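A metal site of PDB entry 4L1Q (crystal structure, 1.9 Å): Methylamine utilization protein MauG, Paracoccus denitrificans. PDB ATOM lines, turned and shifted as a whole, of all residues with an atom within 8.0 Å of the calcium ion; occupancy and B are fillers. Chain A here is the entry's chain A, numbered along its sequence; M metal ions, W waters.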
ATOM      1  N   ARG A  39      -7.209  -3.764  37.551  1.00  0.00           N
ATOM      2  CA  ARG A  39      -6.404  -3.896  36.343  1.00  0.00           C
ATOM      3  C   ARG A  39      -7.223  -4.332  35.127  1.00  0.00           C
ATOM      4  O   ARG A  39      -6.779  -5.208  34.395  1.00  0.00           O
ATOM      5  CB  ARG A  39      -5.262  -4.871  36.486  1.00  0.00           C
ATOM      6  CG  ARG A  39      -4.147  -4.507  35.518  1.00  0.00           C
ATOM      7  CD  ARG A  39      -2.911  -5.308  35.782  1.00  0.00           C
ATOM      8  NE  ARG A  39      -1.736  -4.958  34.974  1.00  0.00           N
ATOM      9  CZ  ARG A  39      -1.462  -5.410  33.760  1.00  0.00           C
ATOM     10  NH1 ARG A  39      -0.339  -5.061  33.126  1.00  0.00           N
ATOM     11  NH2 ARG A  39      -2.339  -6.175  33.103  1.00  0.00           N
ATOM     12  N   THR A  42      -7.632  -8.009  34.666  1.00  0.00           N
ATOM     13  CA  THR A  42      -6.466  -8.763  34.186  1.00  0.00           C
ATOM     14  C   THR A  42      -5.542  -8.962  35.401  1.00  0.00           C
ATOM     15  O   THR A  42      -5.835  -8.433  36.495  1.00  0.00           O
ATOM     16  CB  THR A  42      -5.703  -8.014  33.057  1.00  0.00           C
ATOM     17  OG1 THR A  42      -5.288  -6.712  33.512  1.00  0.00           O
ATOM     18  CG2 THR A  42      -6.555  -7.780  31.897  1.00  0.00           C
ATOM     19  N   ASP A  43      -4.435  -9.674  35.203  1.00  0.00           N
ATOM     20  CA  ASP A  43      -3.642 -10.189  36.312  1.00  0.00           C
ATOM     21  C   ASP A  43      -2.389  -9.310  36.469  1.00  0.00           C
ATOM     22  O   ASP A  43      -1.470  -9.334  35.619  1.00  0.00           O
ATOM     23  CB  ASP A  43      -3.250 -11.636  36.109  1.00  0.00           C
ATOM     24  CG  ASP A  43      -2.621 -12.281  37.366  1.00  0.00           C
ATOM     25  OD1 ASP A  43      -2.420 -11.568  38.429  1.00  0.00           O
ATOM     26  OD2 ASP A  43      -2.383 -13.516  37.326  1.00  0.00           O
ATOM     27  N   LEU A  51       4.345 -11.125  33.372  1.00  0.00           N
ATOM     28  CA  LEU A  51       2.905 -10.874  33.349  1.00  0.00           C
ATOM     29  C   LEU A  51       2.297 -11.502  32.103  1.00  0.00           C
ATOM     30  O   LEU A  51       1.087 -11.310  31.812  1.00  0.00           O
ATOM     31  CB  LEU A  51       2.651  -9.341  33.422  1.00  0.00           C
ATOM     32  CG  LEU A  51       2.112  -8.588  34.645  1.00  0.00           C
ATOM     33  CD1 LEU A  51       2.310  -9.260  35.991  1.00  0.00           C
ATOM     34  CD2 LEU A  51       2.721  -7.182  34.675  1.00  0.00           C
ATOM     35  N   ALA A  52       3.087 -12.247  31.346  1.00  0.00           N
ATOM     36  CA  ALA A  52       2.626 -12.909  30.146  1.00  0.00           C
ATOM     37  C   ALA A  52       1.514 -13.892  30.452  1.00  0.00           C
ATOM     38  O   ALA A  52       0.531 -13.981  29.706  1.00  0.00           O
ATOM     39  CB  ALA A  52       3.742 -13.609  29.430  1.00  0.00           C
ATOM     40  N   ASN A  66      -2.175 -15.499  28.094  1.00  0.00           N
ATOM     41  CA  ASN A  66      -2.332 -14.228  28.849  1.00  0.00           C
ATOM     42  C   ASN A  66      -3.766 -14.178  29.251  1.00  0.00           C
ATOM     43  O   ASN A  66      -4.708 -14.449  28.399  1.00  0.00           O
ATOM     44  CB  ASN A  66      -1.940 -13.052  27.914  1.00  0.00           C
ATOM     45  CG  ASN A  66      -2.040 -11.669  28.553  1.00  0.00           C
ATOM     46  OD1 ASN A  66      -2.736 -10.756  28.043  1.00  0.00           O
ATOM     47  ND2 ASN A  66      -1.240 -11.427  29.635  1.00  0.00           N
ATOM     48  N   THR A  67      -3.978 -13.853  30.508  1.00  0.00           N
ATOM     49  CA  THR A  67      -5.257 -13.568  31.024  1.00  0.00           C
ATOM     50  C   THR A  67      -5.864 -12.301  30.394  1.00  0.00           C
ATOM     51  O   THR A  67      -5.388 -11.216  30.587  1.00  0.00           O
ATOM     52  CB  THR A  67      -5.168 -13.427  32.568  1.00  0.00           C
ATOM     53  OG1 THR A  67      -4.768 -14.694  33.173  1.00  0.00           O
ATOM     54  CG2 THR A  67      -6.541 -12.918  33.128  1.00  0.00           C
ATOM     55  N   PRO A  68      -6.976 -12.443  29.638  1.00  0.00           N
ATOM     56  CA  PRO A  68      -7.698 -11.285  29.089  1.00  0.00           C
ATOM     57  C   PRO A  68      -8.634 -10.537  30.047  1.00  0.00           C
ATOM     58  O   PRO A  68      -9.227 -11.081  30.956  1.00  0.00           O
ATOM     59  CB  PRO A  68      -8.475 -11.917  27.870  1.00  0.00           C
ATOM     60  CG  PRO A  68      -8.785 -13.298  28.352  1.00  0.00           C
ATOM     61  CD  PRO A  68      -7.694 -13.701  29.357  1.00  0.00           C
ATOM     62  N   THR A  69      -8.832  -9.272  29.768  1.00  0.00           N
ATOM     63  CA  THR A  69      -9.879  -8.503  30.365  1.00  0.00           C
ATOM     64  C   THR A  69     -11.218  -9.181  30.210  1.00  0.00           C
ATOM     65  O   THR A  69     -11.457  -9.842  29.206  1.00  0.00           O
ATOM     66  CB  THR A  69     -10.012  -7.144  29.708  1.00  0.00           C
ATOM     67  OG1 THR A  69     -10.924  -6.392  30.486  1.00  0.00           O
ATOM     68  CG2 THR A  69     -10.557  -7.293  28.249  1.00  0.00           C
ATOM     69  N   TRP A  93      -9.400 -17.138  24.079  1.00  0.00           N
ATOM     70  CA  TRP A  93      -8.661 -16.719  22.912  1.00  0.00           C
ATOM     71  C   TRP A  93      -8.852 -17.603  21.695  1.00  0.00           C
ATOM     72  O   TRP A  93      -8.573 -17.159  20.585  1.00  0.00           O
ATOM     73  CB  TRP A  93      -7.183 -16.647  23.206  1.00  0.00           C
ATOM     74  CG  TRP A  93      -6.742 -15.609  24.062  1.00  0.00           C
ATOM     75  CD1 TRP A  93      -6.451 -15.700  25.360  1.00  0.00           C
ATOM     76  CD2 TRP A  93      -6.403 -14.301  23.661  1.00  0.00           C
ATOM     77  NE1 TRP A  93      -5.927 -14.539  25.836  1.00  0.00           N
ATOM     78  CE2 TRP A  93      -5.829 -13.658  24.785  1.00  0.00           C
ATOM     79  CE3 TRP A  93      -6.355 -13.654  22.431  1.00  0.00           C
ATOM     80  CZ2 TRP A  93      -5.408 -12.342  24.762  1.00  0.00           C
ATOM     81  CZ3 TRP A  93      -5.945 -12.335  22.395  1.00  0.00           C
ATOM     82  CH2 TRP A  93      -5.410 -11.707  23.548  1.00  0.00           C
ATOM     83  N   ASN A 271      -9.847  -0.754  26.681  1.00  0.00           N
ATOM     84  CA  ASN A 271      -8.802  -0.858  27.722  1.00  0.00           C
ATOM     85  C   ASN A 271      -7.466  -1.509  27.322  1.00  0.00           C
ATOM     86  O   ASN A 271      -6.657  -1.840  28.197  1.00  0.00           O
ATOM     87  CB  ASN A 271      -9.329  -1.577  28.949  1.00  0.00           C
ATOM     88  CG  ASN A 271     -10.472  -0.842  29.590  1.00  0.00           C
ATOM     89  OD1 ASN A 271     -10.406   0.384  29.846  1.00  0.00           O
ATOM     90  ND2 ASN A 271     -11.547  -1.591  29.893  1.00  0.00           N
ATOM     91  N   VAL A 272      -7.163  -1.573  26.039  1.00  0.00           N
ATOM     92  CA  VAL A 272      -5.948  -2.230  25.647  1.00  0.00           C
ATOM     93  C   VAL A 272      -4.721  -1.548  26.273  1.00  0.00           C
ATOM     94  O   VAL A 272      -3.689  -2.216  26.540  1.00  0.00           O
ATOM     95  CB  VAL A 272      -5.801  -2.360  24.136  1.00  0.00           C
ATOM     96  CG1 VAL A 272      -5.654  -1.029  23.405  1.00  0.00           C
ATOM     97  CG2 VAL A 272      -4.666  -3.295  23.781  1.00  0.00           C
ATOM     98  N   VAL A 274      -4.224  -0.521  29.136  1.00  0.00           N
ATOM     99  CA  VAL A 274      -3.889  -0.904  30.492  1.00  0.00           C
ATOM    100  C   VAL A 274      -3.832  -2.421  30.764  1.00  0.00           C
ATOM    101  O   VAL A 274      -3.720  -2.806  31.925  1.00  0.00           O
ATOM    102  CB  VAL A 274      -4.834  -0.259  31.519  1.00  0.00           C
ATOM    103  CG1 VAL A 274      -4.939   1.231  31.220  1.00  0.00           C
ATOM    104  CG2 VAL A 274      -6.239  -0.893  31.446  1.00  0.00           C
ATOM    105  N   THR A 275      -3.899  -3.243  29.724  1.00  0.00           N
ATOM    106  CA  THR A 275      -3.992  -4.709  29.889  1.00  0.00           C
ATOM    107  C   THR A 275      -2.831  -5.429  29.276  1.00  0.00           C
ATOM    108  O   THR A 275      -2.918  -6.557  28.859  1.00  0.00           O
ATOM    109  CB  THR A 275      -5.308  -5.256  29.276  1.00  0.00           C
ATOM    110  OG1 THR A 275      -5.284  -4.962  27.880  1.00  0.00           O
ATOM    111  CG2 THR A 275      -6.402  -4.610  29.908  1.00  0.00           C
ATOM    112  N   GLY A 276      -1.664  -4.798  29.275  1.00  0.00           N
ATOM    113  CA  GLY A 276      -0.445  -5.440  28.875  1.00  0.00           C
ATOM    114  C   GLY A 276      -0.137  -6.600  29.782  1.00  0.00           C
ATOM    115  O   GLY A 276      -0.616  -6.701  30.923  1.00  0.00           O
ATOM    116  N   PRO A 277       0.697  -7.490  29.300  1.00  0.00           N
ATOM    117  CA  PRO A 277       1.312  -7.601  28.011  1.00  0.00           C
ATOM    118  C   PRO A 277       0.259  -8.068  26.948  1.00  0.00           C
ATOM    119  O   PRO A 277      -0.871  -8.372  27.283  1.00  0.00           O
ATOM    120  CB  PRO A 277       2.363  -8.683  28.200  1.00  0.00           C
ATOM    121  CG  PRO A 277       1.945  -9.435  29.390  1.00  0.00           C
ATOM    122  CD  PRO A 277       1.063  -8.591  30.209  1.00  0.00           C
ATOM    123  N   TYR A 278       0.655  -8.169  25.717  1.00  0.00           N
ATOM    124  CA  TYR A 278      -0.317  -8.269  24.607  1.00  0.00           C
ATOM    125  C   TYR A 278      -0.265  -9.560  23.852  1.00  0.00           C
ATOM    126  O   TYR A 278       0.684 -10.333  23.958  1.00  0.00           O
ATOM    127  CB  TYR A 278      -0.171  -7.031  23.687  1.00  0.00           C
ATOM    128  CG  TYR A 278      -0.434  -5.753  24.456  1.00  0.00           C
ATOM    129  CD1 TYR A 278      -1.684  -5.438  24.899  1.00  0.00           C
ATOM    130  CD2 TYR A 278       0.624  -4.975  24.924  1.00  0.00           C
ATOM    131  CE1 TYR A 278      -1.931  -4.340  25.661  1.00  0.00           C
ATOM    132  CE2 TYR A 278       0.410  -3.859  25.738  1.00  0.00           C
ATOM    133  CZ  TYR A 278      -0.861  -3.533  26.072  1.00  0.00           C
ATOM    134  OH  TYR A 278      -1.102  -2.469  26.820  1.00  0.00           O
ATOM    135  N   MET A 279      -1.338  -9.814  23.061  1.00  0.00           N
ATOM    136  CA  MET A 279      -1.464 -10.992  22.283  1.00  0.00           C
ATOM    137  C   MET A 279      -1.772 -12.147  23.128  1.00  0.00           C
ATOM    138  O   MET A 279      -1.695 -12.094  24.356  1.00  0.00           O
ATOM    139  CB  MET A 279      -0.263 -11.244  21.396  1.00  0.00           C
ATOM    140  CG  MET A 279       0.055 -10.057  20.526  1.00  0.00           C
ATOM    141  SD  MET A 279      -1.354  -9.520  19.536  1.00  0.00           S
ATOM    142  CE  MET A 279      -0.567  -8.209  18.620  1.00  0.00           C
ATOM    143  N   HIS A 280      -2.206 -13.212  22.490  1.00  0.00           N
ATOM    144  CA  HIS A 280      -2.744 -14.298  23.293  1.00  0.00           C
ATOM    145  C   HIS A 280      -1.720 -14.885  24.267  1.00  0.00           C
ATOM    146  O   HIS A 280      -2.085 -15.607  25.173  1.00  0.00           O
ATOM    147  CB  HIS A 280      -3.244 -15.425  22.389  1.00  0.00           C
ATOM    148  CG  HIS A 280      -2.178 -16.057  21.584  1.00  0.00           C
ATOM    149  ND1 HIS A 280      -1.929 -15.731  20.274  1.00  0.00           N
ATOM    150  CD2 HIS A 280      -1.245 -16.988  21.937  1.00  0.00           C
ATOM    151  CE1 HIS A 280      -0.938 -16.482  19.820  1.00  0.00           C
ATOM    152  NE2 HIS A 280      -0.476 -17.218  20.822  1.00  0.00           N
ATOM    153  N   ASN A 281      -0.446 -14.678  24.011  1.00  0.00           N
ATOM    154  CA  ASN A 281       0.628 -15.260  24.874  1.00  0.00           C
ATOM    155  C   ASN A 281       1.393 -14.226  25.671  1.00  0.00           C
ATOM    156  O   ASN A 281       2.487 -14.499  26.234  1.00  0.00           O
ATOM    157  CB  ASN A 281       1.577 -16.102  24.053  1.00  0.00           C
ATOM    158  CG  ASN A 281       2.117 -15.357  22.843  1.00  0.00           C
ATOM    159  OD1 ASN A 281       1.996 -14.132  22.736  1.00  0.00           O
ATOM    160  ND2 ASN A 281       2.661 -16.079  21.938  1.00  0.00           N
ATOM    161  N   GLY A 282       0.827 -13.034  25.711  1.00  0.00           N
ATOM    162  CA  GLY A 282       1.463 -11.899  26.339  1.00  0.00           C
ATOM    163  C   GLY A 282       2.898 -11.732  25.923  1.00  0.00           C
ATOM    164  O   GLY A 282       3.696 -11.322  26.744  1.00  0.00           O
ATOM    165  N   VAL A 283       3.216 -12.037  24.666  1.00  0.00           N
ATOM    166  CA  VAL A 283       4.576 -11.948  24.189  1.00  0.00           C
ATOM    167  C   VAL A 283       5.130 -10.524  24.185  1.00  0.00           C
ATOM    168  O   VAL A 283       6.344 -10.323  24.392  1.00  0.00           O
ATOM    169  CB  VAL A 283       4.808 -12.638  22.818  1.00  0.00           C
ATOM    170  CG1 VAL A 283       3.985 -12.035  21.670  1.00  0.00           C
ATOM    171  CG2 VAL A 283       6.296 -12.590  22.453  1.00  0.00           C
ATOM    172  N   PHE A 284       4.285  -9.541  23.914  1.00  0.00           N
ATOM    173  CA  PHE A 284       4.707  -8.110  23.886  1.00  0.00           C
ATOM    174  C   PHE A 284       4.288  -7.335  25.134  1.00  0.00           C
ATOM    175  O   PHE A 284       3.127  -7.316  25.490  1.00  0.00           O
ATOM    176  CB  PHE A 284       4.185  -7.407  22.613  1.00  0.00           C
ATOM    177  CG  PHE A 284       4.391  -8.184  21.360  1.00  0.00           C
ATOM    178  CD1 PHE A 284       5.640  -8.705  21.047  1.00  0.00           C
ATOM    179  CD2 PHE A 284       3.351  -8.335  20.434  1.00  0.00           C
ATOM    180  CE1 PHE A 284       5.831  -9.409  19.892  1.00  0.00           C
ATOM    181  CE2 PHE A 284       3.555  -9.041  19.283  1.00  0.00           C
ATOM    182  CZ  PHE A 284       4.799  -9.588  19.007  1.00  0.00           C
ATOM    183  N   THR A 285       5.272  -6.721  25.874  1.00  0.00           N
ATOM    184  CA  THR A 285       4.918  -6.015  27.067  1.00  0.00           C
ATOM    185  C   THR A 285       4.401  -4.677  26.722  1.00  0.00           C
ATOM    186  O   THR A 285       3.469  -4.210  27.354  1.00  0.00           O
ATOM    187  CB  THR A 285       6.163  -5.750  28.022  1.00  0.00           C
ATOM    188  OG1 THR A 285       7.066  -4.835  27.379  1.00  0.00           O
ATOM    189  CG2 THR A 285       6.914  -7.041  28.249  1.00  0.00           C
HETATM  190 CA    CA M   1      -3.050  -8.720  27.997  1.00  0.00          CA
HETATM  191  O   HOH W   1      -4.986  -8.922  29.035  1.00  0.00           O
HETATM  192  O   HOH W   2      -4.375  -7.111  26.799  1.00  0.00           O
HETATM  193  O   HOH W   3      -2.163  -8.757  30.214  1.00  0.00           O
HETATM  194  O   HOH W   4      -3.426  -9.662  25.741  1.00  0.00           O
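The backbone NH of Asn 66 sits at hydrogen-bond distance from the backbone carbonyl oxygen of His 280, at 2.9 Å.
The indole nitrogen (NE1) of Trp 93 lies within hydrogen-bond range of the backbone carbonyl oxygen (O) of Asn 66.
O of Ala 52 lies close to ND2 of Asn 66 (3.1 Å).
The backbone carbonyl oxygen (O) of Val 272 sits at hydrogen-bond distance from the side-chain hydroxyl (OG1) of Thr 275 (3.4 Å).
ND2 of Asn 66 sits at hydrogen-bond distance from O of Leu 51 (3.2 Å).
The side-chain hydroxyl (OG1) of Thr 275 sits close to the backbone carbonyl oxygen (O) of Asn 271 (3.4 Å).
Three residues have an atom within 4 Å of the calcium ion: Asn 66, Thr 275 and Pro 277.
OD1 of Asn 66 is bound to the calcium ion (2.1 Å).
Water W1 is bound to the calcium ion (2.2 Å).
The backbone carbonyl oxygen (O) of Pro 277 is bound to the calcium ion (2.3 Å).
O of Thr 275 is bound to the calcium ion, at 2.3 Å.
The calcium ion is bound by water W3 (2.4 Å).
Water W2 binds the calcium ion (2.4 Å).
Water W4 binds the calcium ion (2.5 Å).
Water W3 lies within hydrogen-bond range of the backbone carbonyl oxygen (O) of Gly 276 (2.7 Å) and the side-chain amide nitrogen (ND2) of Asn 66 (2.9 Å).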
